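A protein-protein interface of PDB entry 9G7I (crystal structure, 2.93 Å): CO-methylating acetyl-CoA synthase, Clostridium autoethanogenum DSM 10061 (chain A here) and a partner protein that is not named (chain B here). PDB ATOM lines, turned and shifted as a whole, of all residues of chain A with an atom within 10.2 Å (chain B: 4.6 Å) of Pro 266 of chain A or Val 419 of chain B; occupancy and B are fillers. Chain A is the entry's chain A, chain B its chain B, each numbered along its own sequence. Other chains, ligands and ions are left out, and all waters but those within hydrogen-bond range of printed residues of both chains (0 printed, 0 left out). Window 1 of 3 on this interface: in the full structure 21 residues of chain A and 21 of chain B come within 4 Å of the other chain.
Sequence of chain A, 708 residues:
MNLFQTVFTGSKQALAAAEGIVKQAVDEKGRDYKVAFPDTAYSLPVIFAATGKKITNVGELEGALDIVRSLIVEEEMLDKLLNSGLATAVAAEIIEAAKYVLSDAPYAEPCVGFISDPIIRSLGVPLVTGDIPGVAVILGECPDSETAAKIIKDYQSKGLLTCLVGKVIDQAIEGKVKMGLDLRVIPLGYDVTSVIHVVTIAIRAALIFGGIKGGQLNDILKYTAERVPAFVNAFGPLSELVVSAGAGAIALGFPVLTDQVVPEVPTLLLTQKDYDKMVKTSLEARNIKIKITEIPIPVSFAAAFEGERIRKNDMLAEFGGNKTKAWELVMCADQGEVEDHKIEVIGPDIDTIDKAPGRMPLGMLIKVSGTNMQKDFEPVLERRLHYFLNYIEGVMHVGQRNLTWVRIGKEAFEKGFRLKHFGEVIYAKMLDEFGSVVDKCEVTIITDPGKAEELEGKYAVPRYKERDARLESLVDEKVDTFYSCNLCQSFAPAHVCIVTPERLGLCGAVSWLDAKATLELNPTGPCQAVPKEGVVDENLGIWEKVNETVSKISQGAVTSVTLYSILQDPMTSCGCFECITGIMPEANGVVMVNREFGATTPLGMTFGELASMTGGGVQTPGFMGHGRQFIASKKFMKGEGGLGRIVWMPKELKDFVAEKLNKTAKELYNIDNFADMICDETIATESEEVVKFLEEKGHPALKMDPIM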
ATOM      1  N   LEU A   3     -28.804   3.813   2.299  1.00  0.00           N
ATOM      2  CA  LEU A   3     -28.628   3.166   3.596  1.00  0.00           C
ATOM      3  C   LEU A   3     -27.771   4.019   4.541  1.00  0.00           C
ATOM      4  O   LEU A   3     -28.092   4.140   5.720  1.00  0.00           O
ATOM      5  CB  LEU A   3     -27.983   1.778   3.411  1.00  0.00           C
ATOM      6  CG  LEU A   3     -27.845   0.896   4.657  1.00  0.00           C
ATOM      7  CD1 LEU A   3     -29.165   0.758   5.407  1.00  0.00           C
ATOM      8  CD2 LEU A   3     -27.326  -0.472   4.286  1.00  0.00           C
ATOM      9  N   LEU A  78     -18.014   1.975   4.896  1.00  0.00           N
ATOM     10  CA  LEU A  78     -18.586   0.975   5.844  1.00  0.00           C
ATOM     11  C   LEU A  78     -18.256   1.322   7.301  1.00  0.00           C
ATOM     12  O   LEU A  78     -19.205   1.537   8.076  1.00  0.00           O
ATOM     13  CB  LEU A  78     -18.045  -0.412   5.487  1.00  0.00           C
ATOM     14  CG  LEU A  78     -18.684  -1.576   6.241  1.00  0.00           C
ATOM     15  CD1 LEU A  78     -20.197  -1.423   6.288  1.00  0.00           C
ATOM     16  CD2 LEU A  78     -18.302  -2.905   5.610  1.00  0.00           C
ATOM     17  N   ILE A 250     -25.651  -5.034  13.487  1.00  0.00           N
ATOM     18  CA  ILE A 250     -24.739  -5.478  12.431  1.00  0.00           C
ATOM     19  C   ILE A 250     -23.295  -5.249  12.891  1.00  0.00           C
ATOM     20  O   ILE A 250     -22.443  -6.093  12.620  1.00  0.00           O
ATOM     21  CB  ILE A 250     -25.049  -4.767  11.079  1.00  0.00           C
ATOM     22  CG1 ILE A 250     -26.319  -5.361  10.438  1.00  0.00           C
ATOM     23  CG2 ILE A 250     -23.866  -4.874  10.117  1.00  0.00           C
ATOM     24  CD1 ILE A 250     -26.926  -4.548   9.338  1.00  0.00           C
ATOM     25  N   GLY A 253     -21.883  -7.986  14.683  1.00  0.00           N
ATOM     26  CA  GLY A 253     -21.884  -9.186  13.859  1.00  0.00           C
ATOM     27  C   GLY A 253     -23.215  -9.911  13.805  1.00  0.00           C
ATOM     28  O   GLY A 253     -23.253 -11.075  13.411  1.00  0.00           O
ATOM     29  N   PHE A 254     -24.321  -9.245  14.176  1.00  0.00           N
ATOM     30  CA  PHE A 254     -25.643  -9.881  14.160  1.00  0.00           C
ATOM     31  C   PHE A 254     -26.435  -9.538  12.885  1.00  0.00           C
ATOM     32  O   PHE A 254     -26.683  -8.361  12.626  1.00  0.00           O
ATOM     33  CB  PHE A 254     -26.452  -9.462  15.395  1.00  0.00           C
ATOM     34  CG  PHE A 254     -25.809  -9.737  16.736  1.00  0.00           C
ATOM     35  CD1 PHE A 254     -24.964 -10.823  16.915  1.00  0.00           C
ATOM     36  CD2 PHE A 254     -26.098  -8.944  17.833  1.00  0.00           C
ATOM     37  CE1 PHE A 254     -24.397 -11.082  18.156  1.00  0.00           C
ATOM     38  CE2 PHE A 254     -25.528  -9.207  19.072  1.00  0.00           C
ATOM     39  CZ  PHE A 254     -24.686 -10.277  19.227  1.00  0.00           C
ATOM     40  N   PRO A 255     -26.862 -10.534  12.077  1.00  0.00           N
ATOM     41  CA  PRO A 255     -27.632 -10.202  10.866  1.00  0.00           C
ATOM     42  C   PRO A 255     -29.041  -9.708  11.169  1.00  0.00           C
ATOM     43  O   PRO A 255     -29.714 -10.246  12.044  1.00  0.00           O
ATOM     44  CB  PRO A 255     -27.668 -11.508  10.063  1.00  0.00           C
ATOM     45  CG  PRO A 255     -27.108 -12.551  10.918  1.00  0.00           C
ATOM     46  CD  PRO A 255     -26.666 -11.990  12.224  1.00  0.00           C
ATOM     47  N   VAL A 256     -29.482  -8.690  10.431  1.00  0.00           N
ATOM     48  CA  VAL A 256     -30.803  -8.103  10.589  1.00  0.00           C
ATOM     49  C   VAL A 256     -31.668  -8.564   9.427  1.00  0.00           C
ATOM     50  O   VAL A 256     -31.317  -8.312   8.280  1.00  0.00           O
ATOM     51  CB  VAL A 256     -30.714  -6.561  10.609  1.00  0.00           C
ATOM     52  CG1 VAL A 256     -32.097  -5.944  10.747  1.00  0.00           C
ATOM     53  CG2 VAL A 256     -29.791  -6.072  11.725  1.00  0.00           C
ATOM     54  N   LEU A 257     -32.784  -9.243   9.713  1.00  0.00           N
ATOM     55  CA  LEU A 257     -33.702  -9.722   8.684  1.00  0.00           C
ATOM     56  C   LEU A 257     -35.025  -9.025   8.890  1.00  0.00           C
ATOM     57  O   LEU A 257     -35.583  -9.098   9.979  1.00  0.00           O
ATOM     58  CB  LEU A 257     -33.886 -11.238   8.773  1.00  0.00           C
ATOM     59  CG  LEU A 257     -32.600 -12.065   8.632  1.00  0.00           C
ATOM     60  CD1 LEU A 257     -32.036 -12.450   9.992  1.00  0.00           C
ATOM     61  CD2 LEU A 257     -32.840 -13.299   7.809  1.00  0.00           C
ATOM     62  N   VAL A 262     -35.676  -2.789   2.045  1.00  0.00           N
ATOM     63  CA  VAL A 262     -34.538  -1.976   2.489  1.00  0.00           C
ATOM     64  C   VAL A 262     -33.315  -2.257   1.595  1.00  0.00           C
ATOM     65  O   VAL A 262     -33.285  -3.307   0.961  1.00  0.00           O
ATOM     66  CB  VAL A 262     -34.184  -2.288   3.970  1.00  0.00           C
ATOM     67  CG1 VAL A 262     -35.357  -1.991   4.900  1.00  0.00           C
ATOM     68  CG2 VAL A 262     -33.704  -3.731   4.137  1.00  0.00           C
ATOM     69  N   PRO A 263     -32.283  -1.379   1.546  1.00  0.00           N
ATOM     70  CA  PRO A 263     -31.096  -1.690   0.729  1.00  0.00           C
ATOM     71  C   PRO A 263     -30.337  -2.894   1.305  1.00  0.00           C
ATOM     72  O   PRO A 263     -29.489  -2.742   2.179  1.00  0.00           O
ATOM     73  CB  PRO A 263     -30.261  -0.400   0.804  1.00  0.00           C
ATOM     74  CG  PRO A 263     -31.183   0.639   1.336  1.00  0.00           C
ATOM     75  CD  PRO A 263     -32.121  -0.083   2.229  1.00  0.00           C
ATOM     76  N   GLU A 264     -30.656  -4.093   0.817  1.00  0.00           N
ATOM     77  CA  GLU A 264     -30.069  -5.336   1.300  1.00  0.00           C
ATOM     78  C   GLU A 264     -28.555  -5.383   1.182  1.00  0.00           C
ATOM     79  O   GLU A 264     -28.003  -4.950   0.177  1.00  0.00           O
ATOM     80  CB  GLU A 264     -30.651  -6.527   0.526  1.00  0.00           C
ATOM     81  CG  GLU A 264     -32.088  -6.870   0.871  1.00  0.00           C
ATOM     82  CD  GLU A 264     -32.617  -8.078   0.120  1.00  0.00           C
ATOM     83  OE1 GLU A 264     -32.074  -9.191   0.316  1.00  0.00           O
ATOM     84  OE2 GLU A 264     -33.575  -7.913  -0.668  1.00  0.00           O
ATOM     85  N   VAL A 265     -27.890  -5.944   2.201  1.00  0.00           N
ATOM     86  CA  VAL A 265     -26.443  -6.141   2.227  1.00  0.00           C
ATOM     87  C   VAL A 265     -26.282  -7.638   2.436  1.00  0.00           C
ATOM     88  O   VAL A 265     -26.729  -8.144   3.467  1.00  0.00           O
ATOM     89  CB  VAL A 265     -25.753  -5.357   3.359  1.00  0.00           C
ATOM     90  CG1 VAL A 265     -24.296  -5.787   3.510  1.00  0.00           C
ATOM     91  CG2 VAL A 265     -25.852  -3.859   3.116  1.00  0.00           C
ATOM     92  N   PRO A 266     -25.690  -8.387   1.486  1.00  0.00           N
ATOM     93  CA  PRO A 266     -25.568  -9.844   1.679  1.00  0.00           C
ATOM     94  C   PRO A 266     -25.077 -10.275   3.060  1.00  0.00           C
ATOM     95  O   PRO A 266     -24.142  -9.686   3.597  1.00  0.00           O
ATOM     96  CB  PRO A 266     -24.590 -10.263   0.583  1.00  0.00           C
ATOM     97  CG  PRO A 266     -24.750  -9.255  -0.474  1.00  0.00           C
ATOM     98  CD  PRO A 266     -25.116  -7.963   0.196  1.00  0.00           C
ATOM     99  N   THR A 267     -25.722 -11.309   3.632  1.00  0.00           N
ATOM    100  CA  THR A 267     -25.399 -11.893   4.941  1.00  0.00           C
ATOM    101  C   THR A 267     -25.558 -10.948   6.140  1.00  0.00           C
ATOM    102  O   THR A 267     -25.389 -11.421   7.261  1.00  0.00           O
ATOM    103  CB  THR A 267     -23.972 -12.520   4.962  1.00  0.00           C
ATOM    104  OG1 THR A 267     -22.998 -11.500   5.197  1.00  0.00           O
ATOM    105  CG2 THR A 267     -23.627 -13.272   3.678  1.00  0.00           C
ATOM    106  N   LEU A 268     -25.858  -9.645   5.945  1.00  0.00           N
ATOM    107  CA  LEU A 268     -25.977  -8.721   7.082  1.00  0.00           C
ATOM    108  C   LEU A 268     -27.347  -8.042   7.198  1.00  0.00           C
ATOM    109  O   LEU A 268     -27.857  -7.916   8.305  1.00  0.00           O
ATOM    110  CB  LEU A 268     -24.883  -7.652   7.019  1.00  0.00           C
ATOM    111  CG  LEU A 268     -23.438  -8.156   7.045  1.00  0.00           C
ATOM    112  CD1 LEU A 268     -22.477  -7.039   6.687  1.00  0.00           C
ATOM    113  CD2 LEU A 268     -23.081  -8.758   8.399  1.00  0.00           C
ATOM    114  N   LEU A 269     -27.930  -7.572   6.086  1.00  0.00           N
ATOM    115  CA  LEU A 269     -29.246  -6.919   6.105  1.00  0.00           C
ATOM    116  C   LEU A 269     -30.082  -7.572   5.012  1.00  0.00           C
ATOM    117  O   LEU A 269     -29.758  -7.429   3.840  1.00  0.00           O
ATOM    118  CB  LEU A 269     -29.098  -5.408   5.874  1.00  0.00           C
ATOM    119  CG  LEU A 269     -30.388  -4.586   5.875  1.00  0.00           C
ATOM    120  CD1 LEU A 269     -31.129  -4.713   7.195  1.00  0.00           C
ATOM    121  CD2 LEU A 269     -30.091  -3.122   5.602  1.00  0.00           C
ATOM    122  N   LEU A 270     -31.125  -8.327   5.383  1.00  0.00           N
ATOM    123  CA  LEU A 270     -31.933  -9.053   4.401  1.00  0.00           C
ATOM    124  C   LEU A 270     -33.425  -8.755   4.478  1.00  0.00           C
ATOM    125  O   LEU A 270     -33.916  -8.335   5.517  1.00  0.00           O
ATOM    126  CB  LEU A 270     -31.721 -10.562   4.590  1.00  0.00           C
ATOM    127  CG  LEU A 270     -30.275 -11.037   4.713  1.00  0.00           C
ATOM    128  CD1 LEU A 270     -30.213 -12.428   5.289  1.00  0.00           C
ATOM    129  CD2 LEU A 270     -29.569 -10.979   3.376  1.00  0.00           C
ATOM    130  N   THR A 271     -34.149  -9.001   3.373  1.00  0.00           N
ATOM    131  CA  THR A 271     -35.593  -8.779   3.287  1.00  0.00           C
ATOM    132  C   THR A 271     -36.375 -10.043   2.913  1.00  0.00           C
ATOM    133  O   THR A 271     -36.335 -10.466   1.759  1.00  0.00           O
ATOM    134  CB  THR A 271     -35.915  -7.703   2.226  1.00  0.00           C
ATOM    135  OG1 THR A 271     -35.503  -6.415   2.694  1.00  0.00           O
ATOM    136  CG2 THR A 271     -37.392  -7.658   1.865  1.00  0.00           C
ATOM    137  N   GLU A 284     -30.566 -19.862   9.072  1.00  0.00           N
ATOM    138  CA  GLU A 284     -29.517 -20.003   8.065  1.00  0.00           C
ATOM    139  C   GLU A 284     -28.606 -18.771   8.091  1.00  0.00           C
ATOM    140  O   GLU A 284     -27.383 -18.913   8.094  1.00  0.00           O
ATOM    141  CB  GLU A 284     -30.133 -20.166   6.666  1.00  0.00           C
ATOM    142  CG  GLU A 284     -29.096 -20.217   5.557  1.00  0.00           C
ATOM    143  CD  GLU A 284     -29.673 -20.362   4.167  1.00  0.00           C
ATOM    144  OE1 GLU A 284     -30.752 -20.982   4.035  1.00  0.00           O
ATOM    145  OE2 GLU A 284     -29.044 -19.858   3.208  1.00  0.00           O
ATOM    146  N   ALA A 285     -29.202 -17.566   8.115  1.00  0.00           N
ATOM    147  CA  ALA A 285     -28.459 -16.308   8.131  1.00  0.00           C
ATOM    148  C   ALA A 285     -27.442 -16.219   9.267  1.00  0.00           C
ATOM    149  O   ALA A 285     -26.438 -15.523   9.121  1.00  0.00           O
ATOM    150  CB  ALA A 285     -29.425 -15.138   8.209  1.00  0.00           C
ATOM    151  N   THR A 371     -26.505 -24.671  -6.462  1.00  0.00           N
ATOM    152  CA  THR A 371     -25.136 -24.306  -6.840  1.00  0.00           C
ATOM    153  C   THR A 371     -24.098 -25.277  -6.273  1.00  0.00           C
ATOM    154  O   THR A 371     -24.327 -25.898  -5.233  1.00  0.00           O
ATOM    155  CB  THR A 371     -24.816 -22.858  -6.403  1.00  0.00           C
ATOM    156  OG1 THR A 371     -23.599 -22.431  -7.024  1.00  0.00           O
ATOM    157  CG2 THR A 371     -24.691 -22.711  -4.887  1.00  0.00           C
ATOM    158  N   SER A 436     -24.585 -27.316   1.530  1.00  0.00           N
ATOM    159  CA  SER A 436     -23.509 -26.568   0.887  1.00  0.00           C
ATOM    160  C   SER A 436     -23.437 -26.803  -0.629  1.00  0.00           C
ATOM    161  O   SER A 436     -22.898 -25.958  -1.345  1.00  0.00           O
ATOM    162  CB  SER A 436     -22.172 -26.937   1.521  1.00  0.00           C
ATOM    163  OG  SER A 436     -21.983 -28.343   1.548  1.00  0.00           O
ATOM    164  N   LEU B 416     -20.757 -15.516  -6.086  1.00  0.00           N
ATOM    165  CA  LEU B 416     -21.696 -14.644  -5.384  1.00  0.00           C
ATOM    166  C   LEU B 416     -22.858 -15.447  -4.781  1.00  0.00           C
ATOM    167  O   LEU B 416     -23.460 -14.993  -3.815  1.00  0.00           O
ATOM    168  CB  LEU B 416     -22.254 -13.558  -6.326  1.00  0.00           C
ATOM    169  CG  LEU B 416     -21.283 -12.490  -6.840  1.00  0.00           C
ATOM    170  CD1 LEU B 416     -21.926 -11.667  -7.939  1.00  0.00           C
ATOM    171  CD2 LEU B 416     -20.794 -11.574  -5.715  1.00  0.00           C
ATOM    172  N   ASP B 417     -23.184 -16.624  -5.336  1.00  0.00           N
ATOM    173  CA  ASP B 417     -24.274 -17.450  -4.809  1.00  0.00           C
ATOM    174  C   ASP B 417     -24.027 -17.909  -3.365  1.00  0.00           C
ATOM    175  O   ASP B 417     -24.963 -18.346  -2.701  1.00  0.00           O
ATOM    176  CB  ASP B 417     -24.488 -18.692  -5.694  1.00  0.00           C
ATOM    177  CG  ASP B 417     -25.315 -18.455  -6.941  1.00  0.00           C
ATOM    178  OD1 ASP B 417     -25.671 -17.279  -7.209  1.00  0.00           O
ATOM    179  OD2 ASP B 417     -25.613 -19.444  -7.652  1.00  0.00           O
ATOM    180  N   LYS B 418     -22.788 -17.821  -2.874  1.00  0.00           N
ATOM    181  CA  LYS B 418     -22.483 -18.249  -1.510  1.00  0.00           C
ATOM    182  C   LYS B 418     -22.917 -17.218  -0.474  1.00  0.00           C
ATOM    183  O   LYS B 418     -22.935 -17.539   0.716  1.00  0.00           O
ATOM    184  CB  LYS B 418     -20.993 -18.588  -1.362  1.00  0.00           C
ATOM    185  CG  LYS B 418     -20.447 -19.510  -2.461  1.00  0.00           C
ATOM    186  CD  LYS B 418     -21.080 -20.915  -2.469  1.00  0.00           C
ATOM    187  CE  LYS B 418     -20.883 -21.631  -3.782  1.00  0.00           C
ATOM    188  NZ  LYS B 418     -20.522 -23.058  -3.582  1.00  0.00           N
ATOM    189  N   VAL B 419     -23.279 -15.997  -0.912  1.00  0.00           N
ATOM    190  CA  VAL B 419     -23.744 -14.948  -0.013  1.00  0.00           C
ATOM    191  C   VAL B 419     -25.253 -14.712  -0.192  1.00  0.00           C
ATOM    192  O   VAL B 419     -25.748 -13.652   0.193  1.00  0.00           O
ATOM    193  CB  VAL B 419     -22.926 -13.639  -0.155  1.00  0.00           C
ATOM    194  CG1 VAL B 419     -21.443 -13.899   0.078  1.00  0.00           C
ATOM    195  CG2 VAL B 419     -23.154 -12.965  -1.504  1.00  0.00           C
ATOM    196  N   VAL B 420     -25.963 -15.731  -0.679  1.00  0.00           N
ATOM    197  CA  VAL B 420     -27.416 -15.574  -0.970  1.00  0.00           C
ATOM    198  C   VAL B 420     -28.210 -16.595  -0.145  1.00  0.00           C
ATOM    199  O   VAL B 420     -27.880 -17.793  -0.227  1.00  0.00           O
ATOM    200  CB  VAL B 420     -27.634 -15.740  -2.484  1.00  0.00           C
ATOM    201  CG1 VAL B 420     -29.059 -16.107  -2.826  1.00  0.00           C
ATOM    202  CG2 VAL B 420     -27.199 -14.504  -3.253  1.00  0.00           C
ATOM    203  N   ASN B 421     -29.211 -16.141   0.624  1.00  0.00           N
ATOM    204  CA  ASN B 421     -29.978 -17.061   1.507  1.00  0.00           C
ATOM    205  C   ASN B 421     -30.811 -18.004   0.636  1.00  0.00           C
ATOM    206  O   ASN B 421     -31.349 -17.541  -0.385  1.00  0.00           O
ATOM    207  CB  ASN B 421     -30.849 -16.302   2.512  1.00  0.00           C
ATOM    208  CG  ASN B 421     -31.265 -17.153   3.692  1.00  0.00           C
ATOM    209  OD1 ASN B 421     -31.954 -18.156   3.527  1.00  0.00           O
ATOM    210  ND2 ASN B 421     -30.852 -16.763   4.886  1.00  0.00           N
ATOM    211  N   PRO B 432     -26.428 -10.089  -5.746  1.00  0.00           N
ATOM    212  CA  PRO B 432     -25.540  -9.748  -4.619  1.00  0.00           C
ATOM    213  C   PRO B 432     -24.575  -8.602  -4.917  1.00  0.00           C
ATOM    214  O   PRO B 432     -24.317  -7.783  -4.040  1.00  0.00           O
ATOM    215  CB  PRO B 432     -24.804 -11.061  -4.344  1.00  0.00           C
ATOM    216  CG  PRO B 432     -25.699 -12.103  -4.862  1.00  0.00           C
ATOM    217  CD  PRO B 432     -26.311 -11.520  -6.088  1.00  0.00           C
ATOM    218  N   ASP B 435     -26.610  -5.433  -5.062  1.00  0.00           N
ATOM    219  CA  ASP B 435     -27.010  -5.128  -3.687  1.00  0.00           C
ATOM    220  C   ASP B 435     -25.929  -4.314  -2.967  1.00  0.00           C
ATOM    221  O   ASP B 435     -26.234  -3.247  -2.446  1.00  0.00           O
ATOM    222  CB  ASP B 435     -27.284  -6.422  -2.891  1.00  0.00           C
ATOM    223  CG  ASP B 435     -28.620  -7.085  -3.161  1.00  0.00           C
ATOM    224  OD1 ASP B 435     -29.370  -6.585  -4.039  1.00  0.00           O
ATOM    225  OD2 ASP B 435     -28.919  -8.109  -2.498  1.00  0.00           O
ATOM    226  N   VAL B 436     -24.673  -4.806  -2.931  1.00  0.00           N
ATOM    227  CA  VAL B 436     -23.586  -4.080  -2.255  1.00  0.00           C
ATOM    228  C   VAL B 436     -23.318  -2.738  -2.917  1.00  0.00           C
ATOM    229  O   VAL B 436     -22.944  -1.793  -2.224  1.00  0.00           O
ATOM    230  CB  VAL B 436     -22.266  -4.889  -2.112  1.00  0.00           C
ATOM    231  CG1 VAL B 436     -22.426  -6.043  -1.133  1.00  0.00           C
ATOM    232  CG2 VAL B 436     -21.754  -5.387  -3.459  1.00  0.00           C
ATOM    233  N   LEU B 511     -16.493 -12.245   2.650  1.00  0.00           N
ATOM    234  CA  LEU B 511     -17.760 -12.960   2.490  1.00  0.00           C
ATOM    235  C   LEU B 511     -17.807 -13.780   1.197  1.00  0.00           C
ATOM    236  O   LEU B 511     -18.169 -14.956   1.234  1.00  0.00           O
ATOM    237  CB  LEU B 511     -18.936 -11.967   2.502  1.00  0.00           C
ATOM    238  CG  LEU B 511     -19.118 -11.146   3.775  1.00  0.00           C
ATOM    239  CD1 LEU B 511     -19.963  -9.917   3.509  1.00  0.00           C
ATOM    240  CD2 LEU B 511     -19.743 -11.972   4.874  1.00  0.00           C
ATOM    241  N   VAL B 512     -17.449 -13.167   0.060  1.00  0.00           N
ATOM    242  CA  VAL B 512     -17.477 -13.852  -1.236  1.00  0.00           C
ATOM    243  C   VAL B 512     -16.248 -14.766  -1.429  1.00  0.00           C
ATOM    244  O   VAL B 512     -16.289 -15.655  -2.283  1.00  0.00           O
ATOM    245  CB  VAL B 512     -17.629 -12.845  -2.410  1.00  0.00           C
ATOM    246  CG1 VAL B 512     -17.901 -13.567  -3.725  1.00  0.00           C
ATOM    247  CG2 VAL B 512     -18.741 -11.841  -2.136  1.00  0.00           C
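Of the 11 printed residues of chain B, 7 touch a printed residue of chain A.
Printed residues of chain B that touch a printed residue of chain A: Asp 417, Val 419, Asn 421, Pro 432, Asp 435, Val 436 and Leu 511.
Hydrophobic or aromatic side chains of chain B within 4 Å of the printed part of chain A: Val 419, Val 436 and Leu 511.
Of the 22 printed residues of chain A, 6 touch a printed residue of chain B.
Printed residues of chain A that touch a printed residue of chain B: Glu 264, Pro 266, Thr 267, Glu 284, Ala 285 and Thr 371.
Hydrophobic or aromatic side chains of chain A within 4 Å of the printed part of chain B: Pro 266 and Ala 285.
Along chain A the printed residues that touch a printed residue of chain B span positions 264 to 371.
Among the printed residues, 9 pairs touch across the chains.
The side-chain amide oxygen (OD1) of Asn 421 of chain B lies close to the side-chain carboxylate (OE1) of Glu 284 of chain A (3.1 Å).
Among the printed residues, pairs that only touch across the chains: Thr 267 of chain A with Leu 511 of chain B (3.3 Å), Glu 264 of chain A with Asp 435 of chain B (3.5 Å), Pro 266 of chain A with Val 436 of chain B (3.6 Å), Pro 266 of chain A with Val 419 of chain B (3.6 Å), Thr 371 of chain A with Asp 417 of chain B (3.7 Å), Ala 285 of chain A with Asn 421 of chain B (3.7 Å), Pro 266 of chain A with Pro 432 of chain B (3.9 Å) and Thr 267 of chain A with Val 419 of chain B (3.9 Å).
Of chain B, only Val 419 (3.6 Å), Pro 432 (3.9 Å) and Val 436 (3.6 Å) come within 4 Å of Pro 266 of chain A.
Val 419 of chain B touches just these residues of chain A: Pro 266 and Thr 267.
Pro 432 of chain B touches just one residue of chain A: Pro 266 (3.9 Å).
Leu 511 of chain B touches one residue of chain A.
No residue of chain A comes within 4 Å of Val 512 of chain B.
Printed residues of chain A within 4 Å of Asp 435 of chain B: Glu 264 (3.5 Å).
Printed residues of chain B within 4 Å of Ala 285 of chain A: Asn 421 (3.7 Å).
Of the printed residues of chain B, Glu 264 of chain A touches Asp 435 (3.5 Å).
Of the printed residues of chain B, Thr 267 of chain A touches Val 419 and Leu 511.
Val 265 of chain A touches none of the printed residues of chain B.
The nearest residue of chain B that does not touch Pro 266 of chain A is Asp 435 of chain B (4.1 Å).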
